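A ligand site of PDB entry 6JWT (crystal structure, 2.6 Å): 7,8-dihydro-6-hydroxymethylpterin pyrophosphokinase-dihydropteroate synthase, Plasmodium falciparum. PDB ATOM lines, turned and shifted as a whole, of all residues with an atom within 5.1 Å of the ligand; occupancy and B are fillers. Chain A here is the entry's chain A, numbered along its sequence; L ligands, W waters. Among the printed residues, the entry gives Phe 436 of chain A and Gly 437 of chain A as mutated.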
ATOM      1  N   ASP A 430       0.202  13.308 -10.614  1.00  0.00           N
ATOM      2  CA  ASP A 430      -0.966  12.453 -10.414  1.00  0.00           C
ATOM      3  C   ASP A 430      -1.194  11.744 -11.751  1.00  0.00           C
ATOM      4  O   ASP A 430      -1.705  12.362 -12.687  1.00  0.00           O
ATOM      5  CB  ASP A 430      -2.200  13.276  -9.980  1.00  0.00           C
ATOM      6  CG  ASP A 430      -3.451  12.498  -9.563  1.00  0.00           C
ATOM      7  OD1 ASP A 430      -3.303  11.539  -8.775  1.00  0.00           O
ATOM      8  OD2 ASP A 430      -4.603  12.882 -10.001  1.00  0.00           O
ATOM      9  N   PHE A 436     -12.295   9.361 -15.420  1.00  0.00           N
ATOM     10  CA  PHE A 436     -13.416   9.483 -14.494  1.00  0.00           C
ATOM     11  C   PHE A 436     -14.321  10.659 -14.877  1.00  0.00           C
ATOM     12  O   PHE A 436     -15.336  10.906 -14.208  1.00  0.00           O
ATOM     13  CB  PHE A 436     -12.912   9.577 -13.045  1.00  0.00           C
ATOM     14  CG  PHE A 436     -12.165   8.388 -12.490  1.00  0.00           C
ATOM     15  CD1 PHE A 436     -12.816   7.172 -12.243  1.00  0.00           C
ATOM     16  CD2 PHE A 436     -10.816   8.505 -12.127  1.00  0.00           C
ATOM     17  CE1 PHE A 436     -12.126   6.107 -11.676  1.00  0.00           C
ATOM     18  CE2 PHE A 436     -10.131   7.424 -11.593  1.00  0.00           C
ATOM     19  CZ  PHE A 436     -10.788   6.226 -11.363  1.00  0.00           C
ATOM     20  N   GLY A 437     -13.967  11.349 -15.983  1.00  0.00           N
ATOM     21  CA  GLY A 437     -14.716  12.488 -16.499  1.00  0.00           C
ATOM     22  C   GLY A 437     -16.068  12.077 -17.080  1.00  0.00           C
ATOM     23  O   GLY A 437     -16.299  10.904 -17.299  1.00  0.00           O
ATOM     24  N   PRO A 438     -16.989  13.040 -17.376  1.00  0.00           N
ATOM     25  CA  PRO A 438     -18.371  12.710 -17.737  1.00  0.00           C
ATOM     26  C   PRO A 438     -18.563  12.031 -19.105  1.00  0.00           C
ATOM     27  O   PRO A 438     -17.987  12.464 -20.106  1.00  0.00           O
ATOM     28  CB  PRO A 438     -19.089  14.066 -17.678  1.00  0.00           C
ATOM     29  CG  PRO A 438     -17.995  15.062 -18.009  1.00  0.00           C
ATOM     30  CD  PRO A 438     -16.739  14.489 -17.386  1.00  0.00           C
ATOM     31  N   ASP A 482      -4.115   8.093  -9.374  1.00  0.00           N
ATOM     32  CA  ASP A 482      -5.549   8.277  -9.373  1.00  0.00           C
ATOM     33  C   ASP A 482      -6.238   6.919  -9.626  1.00  0.00           C
ATOM     34  O   ASP A 482      -6.486   6.519 -10.758  1.00  0.00           O
ATOM     35  CB  ASP A 482      -5.888   9.303 -10.449  1.00  0.00           C
ATOM     36  CG  ASP A 482      -7.314   9.782 -10.427  1.00  0.00           C
ATOM     37  OD1 ASP A 482      -8.159   9.112  -9.788  1.00  0.00           O
ATOM     38  OD2 ASP A 482      -7.586  10.815 -11.072  1.00  0.00           O
ATOM     39  N   ASN A 502      -4.750   8.698  -4.745  1.00  0.00           N
ATOM     40  CA  ASN A 502      -5.854   9.587  -5.082  1.00  0.00           C
ATOM     41  C   ASN A 502      -7.064   8.697  -5.388  1.00  0.00           C
ATOM     42  O   ASN A 502      -7.219   8.197  -6.519  1.00  0.00           O
ATOM     43  CB  ASN A 502      -5.461  10.580  -6.188  1.00  0.00           C
ATOM     44  CG  ASN A 502      -6.583  11.495  -6.650  1.00  0.00           C
ATOM     45  OD1 ASN A 502      -7.607  11.654  -5.973  1.00  0.00           O
ATOM     46  ND2 ASN A 502      -6.379  12.106  -7.816  1.00  0.00           N
ATOM     47  N   ILE A 504     -10.821   8.627  -5.744  1.00  0.00           N
ATOM     48  CA  ILE A 504     -11.964   9.495  -5.942  1.00  0.00           C
ATOM     49  C   ILE A 504     -13.257   8.916  -5.359  1.00  0.00           C
ATOM     50  O   ILE A 504     -14.301   9.579  -5.405  1.00  0.00           O
ATOM     51  CB  ILE A 504     -12.129   9.771  -7.448  1.00  0.00           C
ATOM     52  CG1 ILE A 504     -12.282   8.454  -8.212  1.00  0.00           C
ATOM     53  CG2 ILE A 504     -10.963  10.603  -7.979  1.00  0.00           C
ATOM     54  CD1 ILE A 504     -13.302   8.548  -9.295  1.00  0.00           C
ATOM     55  N   VAL A 527      -5.792  11.038  -0.739  1.00  0.00           N
ATOM     56  CA  VAL A 527      -6.769  12.057  -1.035  1.00  0.00           C
ATOM     57  C   VAL A 527      -8.118  11.363  -1.076  1.00  0.00           C
ATOM     58  O   VAL A 527      -8.220  10.320  -1.685  1.00  0.00           O
ATOM     59  CB  VAL A 527      -6.453  12.701  -2.409  1.00  0.00           C
ATOM     60  CG1 VAL A 527      -7.418  13.824  -2.746  1.00  0.00           C
ATOM     61  CG2 VAL A 527      -5.005  13.158  -2.490  1.00  0.00           C
ATOM     62  N   MET A 529     -11.931  12.037  -2.070  1.00  0.00           N
ATOM     63  CA  MET A 529     -12.717  12.987  -2.834  1.00  0.00           C
ATOM     64  C   MET A 529     -14.181  12.608  -2.659  1.00  0.00           C
ATOM     65  O   MET A 529     -14.470  11.430  -2.426  1.00  0.00           O
ATOM     66  CB  MET A 529     -12.309  12.932  -4.316  1.00  0.00           C
ATOM     67  CG  MET A 529     -12.862  14.076  -5.108  1.00  0.00           C
ATOM     68  SD  MET A 529     -12.841  13.724  -6.877  1.00  0.00           S
ATOM     69  CE  MET A 529     -14.294  12.680  -6.975  1.00  0.00           C
ATOM     70  N   MET A 538     -23.465  10.409 -12.701  1.00  0.00           N
ATOM     71  CA  MET A 538     -22.991  11.594 -11.980  1.00  0.00           C
ATOM     72  C   MET A 538     -23.906  12.806 -12.161  1.00  0.00           C
ATOM     73  O   MET A 538     -24.336  13.398 -11.196  1.00  0.00           O
ATOM     74  CB  MET A 538     -21.615  12.026 -12.503  1.00  0.00           C
ATOM     75  CG  MET A 538     -20.474  11.799 -11.557  1.00  0.00           C
ATOM     76  SD  MET A 538     -18.929  12.199 -12.398  1.00  0.00           S
ATOM     77  CE  MET A 538     -19.488  13.534 -13.452  1.00  0.00           C
ATOM     78  N   ASP A 575     -10.963  16.544  -0.704  1.00  0.00           N
ATOM     79  CA  ASP A 575     -11.248  17.106  -2.016  1.00  0.00           C
ATOM     80  C   ASP A 575     -12.761  17.071  -2.200  1.00  0.00           C
ATOM     81  O   ASP A 575     -13.409  16.028  -2.042  1.00  0.00           O
ATOM     82  CB  ASP A 575     -10.451  16.377  -3.090  1.00  0.00           C
ATOM     83  CG  ASP A 575     -10.681  16.843  -4.519  1.00  0.00           C
ATOM     84  OD1 ASP A 575     -11.528  17.752  -4.728  1.00  0.00           O
ATOM     85  OD2 ASP A 575     -10.009  16.303  -5.433  1.00  0.00           O
ATOM     86  N   GLY A 577     -14.424  17.367  -4.870  1.00  0.00           N
ATOM     87  CA  GLY A 577     -14.805  16.748  -6.135  1.00  0.00           C
ATOM     88  C   GLY A 577     -15.620  17.655  -7.063  1.00  0.00           C
ATOM     89  O   GLY A 577     -16.724  17.308  -7.447  1.00  0.00           O
ATOM     90  N   LEU A 578     -15.050  18.791  -7.493  1.00  0.00           N
ATOM     91  CA  LEU A 578     -15.732  19.680  -8.423  1.00  0.00           C
ATOM     92  C   LEU A 578     -16.151  18.895  -9.672  1.00  0.00           C
ATOM     93  O   LEU A 578     -15.396  18.094 -10.212  1.00  0.00           O
ATOM     94  CB  LEU A 578     -14.770  20.807  -8.811  1.00  0.00           C
ATOM     95  CG  LEU A 578     -14.348  21.719  -7.655  1.00  0.00           C
ATOM     96  CD1 LEU A 578     -13.192  22.601  -8.086  1.00  0.00           C
ATOM     97  CD2 LEU A 578     -15.523  22.533  -7.148  1.00  0.00           C
ATOM     98  N   GLY A 579     -17.364  19.146 -10.155  1.00  0.00           N
ATOM     99  CA  GLY A 579     -17.838  18.479 -11.357  1.00  0.00           C
ATOM    100  C   GLY A 579     -18.258  17.019 -11.147  1.00  0.00           C
ATOM    101  O   GLY A 579     -18.632  16.390 -12.107  1.00  0.00           O
ATOM    102  N   PHE A 580     -18.162  16.463  -9.937  1.00  0.00           N
ATOM    103  CA  PHE A 580     -18.616  15.080  -9.720  1.00  0.00           C
ATOM    104  C   PHE A 580     -19.929  15.089  -8.936  1.00  0.00           C
ATOM    105  O   PHE A 580     -19.908  15.259  -7.714  1.00  0.00           O
ATOM    106  CB  PHE A 580     -17.622  14.301  -8.869  1.00  0.00           C
ATOM    107  CG  PHE A 580     -16.340  13.851  -9.520  1.00  0.00           C
ATOM    108  CD1 PHE A 580     -15.235  14.699  -9.570  1.00  0.00           C
ATOM    109  CD2 PHE A 580     -16.240  12.580 -10.071  1.00  0.00           C
ATOM    110  CE1 PHE A 580     -14.041  14.291 -10.156  1.00  0.00           C
ATOM    111  CE2 PHE A 580     -15.042  12.171 -10.665  1.00  0.00           C
ATOM    112  CZ  PHE A 580     -13.953  13.026 -10.702  1.00  0.00           C
ATOM    113  N   HIS A 584     -23.168  23.124 -12.439  1.00  0.00           N
ATOM    114  CA  HIS A 584     -22.072  24.084 -12.508  1.00  0.00           C
ATOM    115  C   HIS A 584     -22.175  25.144 -11.419  1.00  0.00           C
ATOM    116  O   HIS A 584     -21.159  25.555 -10.873  1.00  0.00           O
ATOM    117  CB  HIS A 584     -21.962  24.586 -13.938  1.00  0.00           C
ATOM    118  CG  HIS A 584     -21.734  23.458 -14.882  1.00  0.00           C
ATOM    119  ND1 HIS A 584     -22.197  23.484 -16.194  1.00  0.00           N
ATOM    120  CD2 HIS A 584     -21.146  22.259 -14.689  1.00  0.00           C
ATOM    121  CE1 HIS A 584     -21.860  22.351 -16.796  1.00  0.00           C
ATOM    122  NE2 HIS A 584     -21.214  21.590 -15.890  1.00  0.00           N
ATOM    123  N   PHE A 603      -7.264  19.634  -1.304  1.00  0.00           N
ATOM    124  CA  PHE A 603      -6.796  19.279  -2.628  1.00  0.00           C
ATOM    125  C   PHE A 603      -7.995  19.523  -3.547  1.00  0.00           C
ATOM    126  O   PHE A 603      -9.089  19.053  -3.242  1.00  0.00           O
ATOM    127  CB  PHE A 603      -6.367  17.808  -2.585  1.00  0.00           C
ATOM    128  CG  PHE A 603      -5.866  17.147  -3.853  1.00  0.00           C
ATOM    129  CD1 PHE A 603      -6.663  17.038  -4.981  1.00  0.00           C
ATOM    130  CD2 PHE A 603      -4.606  16.567  -3.883  1.00  0.00           C
ATOM    131  CE1 PHE A 603      -6.187  16.409  -6.120  1.00  0.00           C
ATOM    132  CE2 PHE A 603      -4.116  15.954  -5.029  1.00  0.00           C
ATOM    133  CZ  PHE A 603      -4.910  15.877  -6.149  1.00  0.00           C
ATOM    134  N   ILE A 604      -7.833  20.307  -4.623  1.00  0.00           N
ATOM    135  CA  ILE A 604      -8.945  20.466  -5.535  1.00  0.00           C
ATOM    136  C   ILE A 604      -8.511  20.275  -6.986  1.00  0.00           C
ATOM    137  O   ILE A 604      -7.340  20.476  -7.341  1.00  0.00           O
ATOM    138  CB  ILE A 604      -9.677  21.810  -5.325  1.00  0.00           C
ATOM    139  CG1 ILE A 604      -8.885  23.008  -5.869  1.00  0.00           C
ATOM    140  CG2 ILE A 604     -10.125  21.988  -3.889  1.00  0.00           C
ATOM    141  CD1 ILE A 604      -9.521  24.354  -5.569  1.00  0.00           C
ATOM    142  N   GLY A 605      -9.486  19.906  -7.840  1.00  0.00           N
ATOM    143  CA  GLY A 605      -9.253  19.792  -9.263  1.00  0.00           C
ATOM    144  C   GLY A 605     -10.356  20.494 -10.032  1.00  0.00           C
ATOM    145  O   GLY A 605     -11.475  20.006 -10.081  1.00  0.00           O
ATOM    146  N   ARG A 608      -9.866  22.382 -16.501  1.00  0.00           N
ATOM    147  CA  ARG A 608     -10.514  22.018 -17.747  1.00  0.00           C
ATOM    148  C   ARG A 608     -11.912  21.428 -17.580  1.00  0.00           C
ATOM    149  O   ARG A 608     -12.410  20.805 -18.499  1.00  0.00           O
ATOM    150  CB  ARG A 608      -9.649  21.090 -18.585  1.00  0.00           C
ATOM    151  CG  ARG A 608      -8.331  21.713 -18.995  1.00  0.00           C
ATOM    152  CD  ARG A 608      -7.614  20.858 -20.001  1.00  0.00           C
ATOM    153  NE  ARG A 608      -6.341  21.456 -20.384  1.00  0.00           N
ATOM    154  CZ  ARG A 608      -5.450  20.909 -21.227  1.00  0.00           C
ATOM    155  NH1 ARG A 608      -5.680  19.737 -21.802  1.00  0.00           N
ATOM    156  NH2 ARG A 608      -4.342  21.565 -21.506  1.00  0.00           N
ATOM    157  N   LYS A 609     -12.591  21.675 -16.452  1.00  0.00           N
ATOM    158  CA  LYS A 609     -13.928  21.120 -16.283  1.00  0.00           C
ATOM    159  C   LYS A 609     -14.969  22.075 -16.868  1.00  0.00           C
ATOM    160  O   LYS A 609     -14.730  23.270 -17.015  1.00  0.00           O
ATOM    161  CB  LYS A 609     -14.174  20.747 -14.813  1.00  0.00           C
ATOM    162  CG  LYS A 609     -13.130  19.823 -14.220  1.00  0.00           C
ATOM    163  CD  LYS A 609     -13.475  19.300 -12.842  1.00  0.00           C
ATOM    164  CE  LYS A 609     -12.707  18.024 -12.589  1.00  0.00           C
ATOM    165  NZ  LYS A 609     -12.527  17.713 -11.149  1.00  0.00           N
ATOM    166  N   ARG A 610     -16.140  21.537 -17.191  1.00  0.00           N
ATOM    167  CA  ARG A 610     -17.179  22.275 -17.890  1.00  0.00           C
ATOM    168  C   ARG A 610     -17.604  23.517 -17.121  1.00  0.00           C
ATOM    169  O   ARG A 610     -17.987  24.526 -17.714  1.00  0.00           O
ATOM    170  CB  ARG A 610     -18.396  21.379 -18.120  1.00  0.00           C
ATOM    171  CG  ARG A 610     -18.127  20.187 -19.025  1.00  0.00           C
ATOM    172  CD  ARG A 610     -19.132  19.059 -18.868  1.00  0.00           C
ATOM    173  NE  ARG A 610     -19.143  18.498 -17.517  1.00  0.00           N
ATOM    174  CZ  ARG A 610     -20.106  17.706 -17.019  1.00  0.00           C
ATOM    175  NH1 ARG A 610     -21.137  17.343 -17.767  1.00  0.00           N
ATOM    176  NH2 ARG A 610     -20.009  17.261 -15.778  1.00  0.00           N
ATOM    177  N   ARG A 686      -4.936  20.521  -8.766  1.00  0.00           N
ATOM    178  CA  ARG A 686      -4.650  19.440  -9.711  1.00  0.00           C
ATOM    179  C   ARG A 686      -4.862  19.974 -11.118  1.00  0.00           C
ATOM    180  O   ARG A 686      -5.988  20.258 -11.530  1.00  0.00           O
ATOM    181  CB  ARG A 686      -5.568  18.233  -9.424  1.00  0.00           C
ATOM    182  CG  ARG A 686      -5.052  16.925 -10.008  1.00  0.00           C
ATOM    183  CD  ARG A 686      -5.925  15.678  -9.873  1.00  0.00           C
ATOM    184  NE  ARG A 686      -6.849  15.869 -10.968  1.00  0.00           N
ATOM    185  CZ  ARG A 686      -7.023  15.051 -11.987  1.00  0.00           C
ATOM    186  NH1 ARG A 686      -6.348  13.917 -12.041  1.00  0.00           N
ATOM    187  NH2 ARG A 686      -7.891  15.386 -12.919  1.00  0.00           N
HETATM  188  C1  LIG L   1     -10.517  15.633  -9.033  1.00  0.00           C
HETATM  189  C2  LIG L   1     -10.359  14.741 -10.142  1.00  0.00           C
HETATM  190  C3  LIG L   1      -9.591  13.514  -9.906  1.00  0.00           C
HETATM  191  N1  LIG L   1     -10.907  15.047 -11.354  1.00  0.00           N
HETATM  192  C4  LIG L   1      -9.293  14.214  -7.688  1.00  0.00           C
HETATM  193  N2  LIG L   1      -9.069  13.325  -8.677  1.00  0.00           N
HETATM  194  C5  LIG L   1     -10.724  14.123 -12.335  1.00  0.00           C
HETATM  195  N3  LIG L   1      -8.787  13.951  -6.446  1.00  0.00           N
HETATM  196  C6  LIG L   1      -9.961  12.948 -12.119  1.00  0.00           C
HETATM  197  C7  LIG L   1     -16.337  17.907 -15.873  1.00  0.00           C
HETATM  198  O1  LIG L   1     -15.943  18.429 -16.938  1.00  0.00           O
HETATM  199  O2  LIG L   1     -11.220  16.732  -9.278  1.00  0.00           O
HETATM  200  N4  LIG L   1      -9.994  15.359  -7.860  1.00  0.00           N
HETATM  201  N5  LIG L   1      -9.425  12.642 -10.935  1.00  0.00           N
HETATM  202  C8  LIG L   1     -11.328  14.399 -13.692  1.00  0.00           C
HETATM  203  N6  LIG L   1     -12.778  14.127 -13.603  1.00  0.00           N
HETATM  204  C9  LIG L   1     -13.684  15.010 -14.136  1.00  0.00           C
HETATM  205  C10 LIG L   1     -14.918  15.273 -13.506  1.00  0.00           C
HETATM  206  C11 LIG L   1     -13.363  15.674 -15.332  1.00  0.00           C
HETATM  207  C12 LIG L   1     -15.823  16.204 -14.056  1.00  0.00           C
HETATM  208  C13 LIG L   1     -14.255  16.615 -15.845  1.00  0.00           C
HETATM  209  C14 LIG L   1     -15.461  16.874 -15.222  1.00  0.00           C
HETATM  210  O3  LIG L   1     -17.405  18.320 -15.340  1.00  0.00           O
HETATM  211  O   HOH W   1     -11.977  18.385  -7.317  1.00  0.00           O
HETATM  212  O   HOH W   2     -17.858  20.875 -14.125  1.00  0.00           O
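NH2 of Arg 686 sits close to N1 of the ligand.
An oxygen (O2) of the ligand is in hydrogen-bond range of the backbone carbonyl oxygen (O) of Gly 605.
The side-chain amino group (NZ) of Lys 609 lies within hydrogen-bond range of an oxygen (O2) of the ligand (2.5 Å).
The side-chain amide oxygen (OD1) of Asn 502 lies within hydrogen-bond range of a nitrogen (N3) of the ligand, at 2.6 Å.
O1 of the ligand lies within hydrogen-bond range of N of Arg 610, 3.1 Å away.
The guanidinium group (NE) of Arg 610 lies within salt-bridge range of an oxygen (O3) of the ligand, 2.8 Å away.
The side-chain carboxylate (OD2) of Asp 482 is in hydrogen-bond range of a nitrogen (N5) of the ligand (2.6 Å).
OD2 of Asp 575 is in hydrogen-bond range of N4 of the ligand, at 2.6 Å.
The side-chain amino group of Lys 609 lies within hydrogen-bond range of the backbone carbonyl oxygen of Gly 605 (2.7 Å).
The backbone NH of Arg 686 lies within hydrogen-bond range of the backbone carbonyl oxygen of Ile 604 (2.8 Å).
The backbone NH of Gly 577 lies within hydrogen-bond range of the side-chain carboxylate of Asp 575, 2.9 Å away.
The side-chain carboxylate (OD2) of Asp 482 is in salt-bridge range of the guanidinium group (NH1) of Arg 686 (3.5 Å).
The side-chain amino group (NZ) of Lys 609 sits at hydrogen-bond distance from the backbone carbonyl oxygen (O) of Leu 578 (3.0 Å).
The guanidinium group of Arg 686 lies within salt-bridge range of the side-chain carboxylate of Asp 430 (2.9 Å).
ND2 of Asn 502 sits at hydrogen-bond distance from OD2 of Asp 430 (2.9 Å).
The side-chain sulfur (SD) of Met 529 lies close to a nitrogen (N4) of the ligand (3.4 Å).
Residues that only touch the ligand: Gly 437, Pro 438, Ile 504, Val 527, Gly 579, Phe 580 and Phe 603.
The nearest printed residue that does not touch the ligand is Phe 436 (4.004 Å).
Water W1 lies within hydrogen-bond range of O2 of the ligand (2.7 Å), OD1 of Asp 575 (2.7 Å), N of Gly 605 (3.0 Å) and N of Leu 578 (3.1 Å).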
